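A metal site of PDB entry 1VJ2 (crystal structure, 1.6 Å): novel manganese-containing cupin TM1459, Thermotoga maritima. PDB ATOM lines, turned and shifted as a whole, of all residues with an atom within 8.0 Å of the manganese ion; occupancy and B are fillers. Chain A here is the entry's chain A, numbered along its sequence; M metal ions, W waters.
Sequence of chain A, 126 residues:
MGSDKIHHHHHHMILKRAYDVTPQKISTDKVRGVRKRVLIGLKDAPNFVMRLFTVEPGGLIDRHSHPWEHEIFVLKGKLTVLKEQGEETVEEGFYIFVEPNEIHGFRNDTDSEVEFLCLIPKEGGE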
ATOM      1  N   ARG A  51     -11.656  -1.014 -25.296  1.00  0.00           N
ATOM      2  CA  ARG A  51     -11.139  -1.548 -24.034  1.00  0.00           C
ATOM      3  C   ARG A  51     -12.110  -2.576 -23.459  1.00  0.00           C
ATOM      4  O   ARG A  51     -13.299  -2.568 -23.708  1.00  0.00           O
ATOM      5  CB  ARG A  51     -10.915  -0.452 -22.990  1.00  0.00           C
ATOM      6  CG  ARG A  51     -10.120   0.761 -23.506  1.00  0.00           C
ATOM      7  CD  ARG A  51     -10.988   1.916 -23.826  1.00  0.00           C
ATOM      8  NE  ARG A  51     -11.055   2.814 -22.668  1.00  0.00           N
ATOM      9  CZ  ARG A  51     -12.147   3.435 -22.264  1.00  0.00           C
ATOM     10  NH1 ARG A  51     -13.279   3.271 -22.889  1.00  0.00           N
ATOM     11  NH2 ARG A  51     -12.090   4.219 -21.210  1.00  0.00           N
ATOM     12  N   PHE A  53     -13.059  -3.926 -19.608  1.00  0.00           N
ATOM     13  CA  PHE A  53     -12.996  -3.635 -18.178  1.00  0.00           C
ATOM     14  C   PHE A  53     -13.570  -4.812 -17.410  1.00  0.00           C
ATOM     15  O   PHE A  53     -14.611  -5.340 -17.801  1.00  0.00           O
ATOM     16  CB  PHE A  53     -13.847  -2.392 -17.876  1.00  0.00           C
ATOM     17  CG  PHE A  53     -13.137  -1.124 -18.214  1.00  0.00           C
ATOM     18  CD1 PHE A  53     -12.284  -0.591 -17.328  1.00  0.00           C
ATOM     19  CD2 PHE A  53     -13.346  -0.513 -19.429  1.00  0.00           C
ATOM     20  CE1 PHE A  53     -11.629   0.542 -17.615  1.00  0.00           C
ATOM     21  CE2 PHE A  53     -12.654   0.622 -19.753  1.00  0.00           C
ATOM     22  CZ  PHE A  53     -11.818   1.165 -18.802  1.00  0.00           C
ATOM     23  N   ILE A  61     -16.234   2.467 -10.276  1.00  0.00           N
ATOM     24  CA  ILE A  61     -15.727   3.607 -11.055  1.00  0.00           C
ATOM     25  C   ILE A  61     -16.654   4.746 -10.722  1.00  0.00           C
ATOM     26  O   ILE A  61     -17.786   4.813 -11.235  1.00  0.00           O
ATOM     27  CB  ILE A  61     -15.668   3.330 -12.601  1.00  0.00           C
ATOM     28  CG1 ILE A  61     -14.666   2.231 -12.971  1.00  0.00           C
ATOM     29  CG2 ILE A  61     -15.321   4.632 -13.331  1.00  0.00           C
ATOM     30  CD1 ILE A  61     -14.910   1.606 -14.318  1.00  0.00           C
ATOM     31  N   ASP A  62     -16.181   5.687  -9.923  1.00  0.00           N
ATOM     32  CA  ASP A  62     -17.078   6.696  -9.399  1.00  0.00           C
ATOM     33  C   ASP A  62     -17.468   7.681 -10.475  1.00  0.00           C
ATOM     34  O   ASP A  62     -16.869   7.758 -11.534  1.00  0.00           O
ATOM     35  CB  ASP A  62     -16.474   7.393  -8.180  1.00  0.00           C
ATOM     36  CG  ASP A  62     -17.521   7.780  -7.149  1.00  0.00           C
ATOM     37  OD1 ASP A  62     -18.737   7.543  -7.335  1.00  0.00           O
ATOM     38  OD2 ASP A  62     -17.212   8.325  -6.107  1.00  0.00           O
ATOM     39  N   ARG A  63     -18.496   8.453 -10.168  1.00  0.00           N
ATOM     40  CA  ARG A  63     -19.088   9.399 -11.090  1.00  0.00           C
ATOM     41  C   ARG A  63     -18.114  10.433 -11.597  1.00  0.00           C
ATOM     42  O   ARG A  63     -17.304  10.987 -10.832  1.00  0.00           O
ATOM     43  CB  ARG A  63     -20.290  10.094 -10.449  1.00  0.00           C
ATOM     44  CG  ARG A  63     -21.511   9.216 -10.246  1.00  0.00           C
ATOM     45  CD  ARG A  63     -22.699  10.011  -9.633  1.00  0.00           C
ATOM     46  NE  ARG A  63     -23.948   9.275  -9.545  1.00  0.00           N
ATOM     47  CZ  ARG A  63     -24.233   8.365  -8.615  1.00  0.00           C
ATOM     48  NH1 ARG A  63     -23.355   8.035  -7.673  1.00  0.00           N
ATOM     49  NH2 ARG A  63     -25.419   7.770  -8.642  1.00  0.00           N
ATOM     50  N   HIS A  64     -18.197  10.702 -12.889  1.00  0.00           N
ATOM     51  CA  HIS A  64     -17.300  11.620 -13.535  1.00  0.00           C
ATOM     52  C   HIS A  64     -17.931  11.998 -14.864  1.00  0.00           C
ATOM     53  O   HIS A  64     -18.896  11.395 -15.241  1.00  0.00           O
ATOM     54  CB  HIS A  64     -15.952  10.952 -13.765  1.00  0.00           C
ATOM     55  CG  HIS A  64     -16.013   9.773 -14.695  1.00  0.00           C
ATOM     56  ND1 HIS A  64     -16.373   8.503 -14.283  1.00  0.00           N
ATOM     57  CD2 HIS A  64     -15.801   9.686 -16.030  1.00  0.00           C
ATOM     58  CE1 HIS A  64     -16.358   7.687 -15.316  1.00  0.00           C
ATOM     59  NE2 HIS A  64     -15.995   8.374 -16.387  1.00  0.00           N
ATOM     60  N   SER A  65     -17.374  12.983 -15.556  1.00  0.00           N
ATOM     61  CA  SER A  65     -17.748  13.233 -16.931  1.00  0.00           C
ATOM     62  C   SER A  65     -16.546  13.705 -17.754  1.00  0.00           C
ATOM     63  O   SER A  65     -15.491  14.048 -17.208  1.00  0.00           O
ATOM     64  CB  SER A  65     -18.866  14.272 -17.011  1.00  0.00           C
ATOM     65  OG  SER A  65     -18.448  15.531 -16.559  1.00  0.00           O
ATOM     66  N   HIS A  66     -16.740  13.711 -19.067  1.00  0.00           N
ATOM     67  CA  HIS A  66     -15.699  14.053 -20.032  1.00  0.00           C
ATOM     68  C   HIS A  66     -16.405  14.369 -21.357  1.00  0.00           C
ATOM     69  O   HIS A  66     -17.462  13.776 -21.646  1.00  0.00           O
ATOM     70  CB  HIS A  66     -14.679  12.874 -20.195  1.00  0.00           C
ATOM     71  CG  HIS A  66     -15.299  11.512 -20.213  1.00  0.00           C
ATOM     72  ND1 HIS A  66     -16.085  11.055 -21.254  1.00  0.00           N
ATOM     73  CD2 HIS A  66     -15.210  10.490 -19.328  1.00  0.00           C
ATOM     74  CE1 HIS A  66     -16.480   9.823 -20.986  1.00  0.00           C
ATOM     75  NE2 HIS A  66     -15.977   9.467 -19.815  1.00  0.00           N
ATOM     76  N   TRP A  68     -16.454  13.362 -24.277  1.00  0.00           N
ATOM     77  CA  TRP A  68     -16.604  12.368 -25.338  1.00  0.00           C
ATOM     78  C   TRP A  68     -17.516  11.252 -24.873  1.00  0.00           C
ATOM     79  O   TRP A  68     -17.650  10.980 -23.664  1.00  0.00           O
ATOM     80  CB  TRP A  68     -15.229  11.808 -25.768  1.00  0.00           C
ATOM     81  CG  TRP A  68     -14.479  11.205 -24.662  1.00  0.00           C
ATOM     82  CD1 TRP A  68     -14.580   9.924 -24.207  1.00  0.00           C
ATOM     83  CD2 TRP A  68     -13.482  11.842 -23.855  1.00  0.00           C
ATOM     84  NE1 TRP A  68     -13.734   9.713 -23.151  1.00  0.00           N
ATOM     85  CE2 TRP A  68     -13.027  10.880 -22.924  1.00  0.00           C
ATOM     86  CE3 TRP A  68     -12.932  13.130 -23.814  1.00  0.00           C
ATOM     87  CZ2 TRP A  68     -12.061  11.162 -21.960  1.00  0.00           C
ATOM     88  CZ3 TRP A  68     -11.953  13.413 -22.862  1.00  0.00           C
ATOM     89  CH2 TRP A  68     -11.520  12.425 -21.962  1.00  0.00           C
ATOM     90  N   GLU A  69     -18.118  10.579 -25.846  1.00  0.00           N
ATOM     91  CA  GLU A  69     -19.082   9.528 -25.590  1.00  0.00           C
ATOM     92  C   GLU A  69     -18.436   8.204 -25.174  1.00  0.00           C
ATOM     93  O   GLU A  69     -17.265   8.020 -25.359  1.00  0.00           O
ATOM     94  CB  GLU A  69     -19.936   9.343 -26.866  1.00  0.00           C
ATOM     95  CG  GLU A  69     -19.234   8.680 -28.042  1.00  0.00           C
ATOM     96  CD  GLU A  69     -18.497   9.621 -28.989  1.00  0.00           C
ATOM     97  OE1 GLU A  69     -18.200  10.822 -28.643  1.00  0.00           O
ATOM     98  OE2 GLU A  69     -18.223   9.119 -30.104  1.00  0.00           O
ATOM     99  N   HIS A  70     -19.246   7.295 -24.628  1.00  0.00           N
ATOM    100  CA  HIS A  70     -18.900   5.889 -24.399  1.00  0.00           C
ATOM    101  C   HIS A  70     -19.938   5.048 -25.122  1.00  0.00           C
ATOM    102  O   HIS A  70     -21.103   5.321 -25.006  1.00  0.00           O
ATOM    103  CB  HIS A  70     -19.042   5.542 -22.927  1.00  0.00           C
ATOM    104  CG  HIS A  70     -17.929   6.023 -22.066  1.00  0.00           C
ATOM    105  ND1 HIS A  70     -16.605   5.670 -22.273  1.00  0.00           N
ATOM    106  CD2 HIS A  70     -17.937   6.780 -20.948  1.00  0.00           C
ATOM    107  CE1 HIS A  70     -15.856   6.231 -21.334  1.00  0.00           C
ATOM    108  NE2 HIS A  70     -16.652   6.877 -20.493  1.00  0.00           N
ATOM    109  N   ILE A  72     -20.773   1.071 -24.908  1.00  0.00           N
ATOM    110  CA  ILE A  72     -20.482   0.006 -23.983  1.00  0.00           C
ATOM    111  C   ILE A  72     -21.322  -1.209 -24.287  1.00  0.00           C
ATOM    112  O   ILE A  72     -22.524  -1.122 -24.705  1.00  0.00           O
ATOM    113  CB  ILE A  72     -20.729   0.445 -22.554  1.00  0.00           C
ATOM    114  CG1 ILE A  72     -19.675   1.430 -22.113  1.00  0.00           C
ATOM    115  CG2 ILE A  72     -20.827  -0.759 -21.541  1.00  0.00           C
ATOM    116  CD1 ILE A  72     -20.122   2.350 -21.090  1.00  0.00           C
ATOM    117  N   VAL A  98     -23.406   6.491 -23.487  1.00  0.00           N
ATOM    118  CA  VAL A  98     -23.292   7.669 -22.651  1.00  0.00           C
ATOM    119  C   VAL A  98     -22.905   8.849 -23.552  1.00  0.00           C
ATOM    120  O   VAL A  98     -21.909   8.830 -24.261  1.00  0.00           O
ATOM    121  CB  VAL A  98     -22.212   7.521 -21.563  1.00  0.00           C
ATOM    122  CG1 VAL A  98     -22.292   8.698 -20.585  1.00  0.00           C
ATOM    123  CG2 VAL A  98     -22.363   6.172 -20.838  1.00  0.00           C
ATOM    124  N   GLU A 102     -22.064  13.610 -20.013  1.00  0.00           N
ATOM    125  CA  GLU A 102     -23.127  13.068 -19.181  1.00  0.00           C
ATOM    126  C   GLU A 102     -22.442  12.387 -18.014  1.00  0.00           C
ATOM    127  O   GLU A 102     -21.467  11.644 -18.185  1.00  0.00           O
ATOM    128  CB  GLU A 102     -23.997  12.097 -19.975  1.00  0.00           C
ATOM    129  CG  GLU A 102     -25.085  11.410 -19.169  1.00  0.00           C
ATOM    130  CD  GLU A 102     -26.126  10.766 -20.043  1.00  0.00           C
ATOM    131  OE1 GLU A 102     -25.776  10.246 -21.134  1.00  0.00           O
ATOM    132  OE2 GLU A 102     -27.324  10.757 -19.639  1.00  0.00           O
ATOM    133  N   ILE A 103     -22.911  12.690 -16.819  1.00  0.00           N
ATOM    134  CA  ILE A 103     -22.334  12.165 -15.610  1.00  0.00           C
ATOM    135  C   ILE A 103     -22.557  10.642 -15.606  1.00  0.00           C
ATOM    136  O   ILE A 103     -23.678  10.163 -15.861  1.00  0.00           O
ATOM    137  CB  ILE A 103     -22.979  12.884 -14.399  1.00  0.00           C
ATOM    138  CG1 ILE A 103     -22.347  14.270 -14.206  1.00  0.00           C
ATOM    139  CG2 ILE A 103     -22.851  12.106 -13.136  1.00  0.00           C
ATOM    140  CD1 ILE A 103     -23.149  15.130 -13.301  1.00  0.00           C
ATOM    141  N   HIS A 104     -21.487   9.877 -15.370  1.00  0.00           N
ATOM    142  CA  HIS A 104     -21.623   8.420 -15.300  1.00  0.00           C
ATOM    143  C   HIS A 104     -20.546   7.791 -14.450  1.00  0.00           C
ATOM    144  O   HIS A 104     -19.494   8.418 -14.147  1.00  0.00           O
ATOM    145  CB  HIS A 104     -21.545   7.827 -16.702  1.00  0.00           C
ATOM    146  CG  HIS A 104     -20.251   8.138 -17.373  1.00  0.00           C
ATOM    147  ND1 HIS A 104     -19.946   9.412 -17.823  1.00  0.00           N
ATOM    148  CD2 HIS A 104     -19.148   7.380 -17.605  1.00  0.00           C
ATOM    149  CE1 HIS A 104     -18.720   9.401 -18.322  1.00  0.00           C
ATOM    150  NE2 HIS A 104     -18.218   8.191 -18.194  1.00  0.00           N
ATOM    151  N   GLY A 105     -20.793   6.536 -14.095  1.00  0.00           N
ATOM    152  CA  GLY A 105     -19.857   5.703 -13.340  1.00  0.00           C
ATOM    153  C   GLY A 105     -20.370   4.282 -13.248  1.00  0.00           C
ATOM    154  O   GLY A 105     -21.423   3.994 -13.804  1.00  0.00           O
ATOM    155  N   PHE A 106     -19.637   3.395 -12.590  1.00  0.00           N
ATOM    156  CA  PHE A 106     -20.016   1.953 -12.531  1.00  0.00           C
ATOM    157  C   PHE A 106     -19.675   1.306 -11.197  1.00  0.00           C
ATOM    158  O   PHE A 106     -18.710   1.699 -10.518  1.00  0.00           O
ATOM    159  CB  PHE A 106     -19.326   1.155 -13.655  1.00  0.00           C
ATOM    160  CG  PHE A 106     -19.463   1.789 -14.992  1.00  0.00           C
ATOM    161  CD1 PHE A 106     -20.566   1.557 -15.787  1.00  0.00           C
ATOM    162  CD2 PHE A 106     -18.507   2.678 -15.429  1.00  0.00           C
ATOM    163  CE1 PHE A 106     -20.707   2.189 -17.016  1.00  0.00           C
ATOM    164  CE2 PHE A 106     -18.649   3.294 -16.683  1.00  0.00           C
ATOM    165  CZ  PHE A 106     -19.749   3.040 -17.453  1.00  0.00           C
ATOM    166  N   CYS A 118     -15.866  -1.244 -23.609  1.00  0.00           N
ATOM    167  CA  CYS A 118     -16.054   0.173 -23.618  1.00  0.00           C
ATOM    168  C   CYS A 118     -15.193   0.744 -24.743  1.00  0.00           C
ATOM    169  O   CYS A 118     -13.966   0.492 -24.837  1.00  0.00           O
ATOM    170  CB  CYS A 118     -15.716   0.799 -22.284  1.00  0.00           C
ATOM    171  SG  CYS A 118     -16.034   2.585 -22.234  1.00  0.00           S
ATOM    172  N   ILE A 120     -14.468   4.400 -27.083  1.00  0.00           N
ATOM    173  CA  ILE A 120     -14.431   5.869 -27.007  1.00  0.00           C
ATOM    174  C   ILE A 120     -13.716   6.394 -28.269  1.00  0.00           C
ATOM    175  O   ILE A 120     -12.890   5.672 -28.835  1.00  0.00           O
ATOM    176  CB  ILE A 120     -13.702   6.361 -25.726  1.00  0.00           C
ATOM    177  CG1 ILE A 120     -12.313   5.713 -25.623  1.00  0.00           C
ATOM    178  CG2 ILE A 120     -14.530   5.989 -24.467  1.00  0.00           C
ATOM    179  CD1 ILE A 120     -11.318   6.401 -24.718  1.00  0.00           C
HETATM  180 MN    MN M   1     -16.152   7.737 -18.475  1.00  0.00          MN
HETATM  181  O   HOH W   1     -14.213   7.090 -18.716  1.00  0.00           O
HETATM  182  O   HOH W   2     -16.066   5.678 -17.589  1.00  0.00           O
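O of His 70 sits at hydrogen-bond distance from N of Val 98 (3.0 Å).
O of Asp 62 is in hydrogen-bond range of ND1 of His 64.
The backbone carbonyl oxygen (O) of Glu 102 is in hydrogen-bond range of a ring nitrogen (ND1) of His 104 (2.7 Å).
A ring nitrogen (ND1) of His 66 lies within hydrogen-bond range of the backbone carbonyl oxygen (O) of Trp 68, 2.9 Å away.
A ring nitrogen (ND1) of His 70 sits at hydrogen-bond distance from the side-chain sulfur (SG) of Cys 118 (3.1 Å).
Four residues have an atom within 4 Å of the manganese ion: His 64, His 66, His 70 and His 104.
Along chain A the residues within 4 Å of the manganese ion span positions 64 to 104.
The manganese ion is bound by water W1 (2.1 Å), a ring nitrogen (NE2) of His 104 (2.1 Å), a ring nitrogen (NE2) of His 64 (2.2 Å), a ring nitrogen (NE2) of His 66 (2.2 Å), water W2 (2.2 Å) and a ring nitrogen (NE2) of His 70 (2.2 Å).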
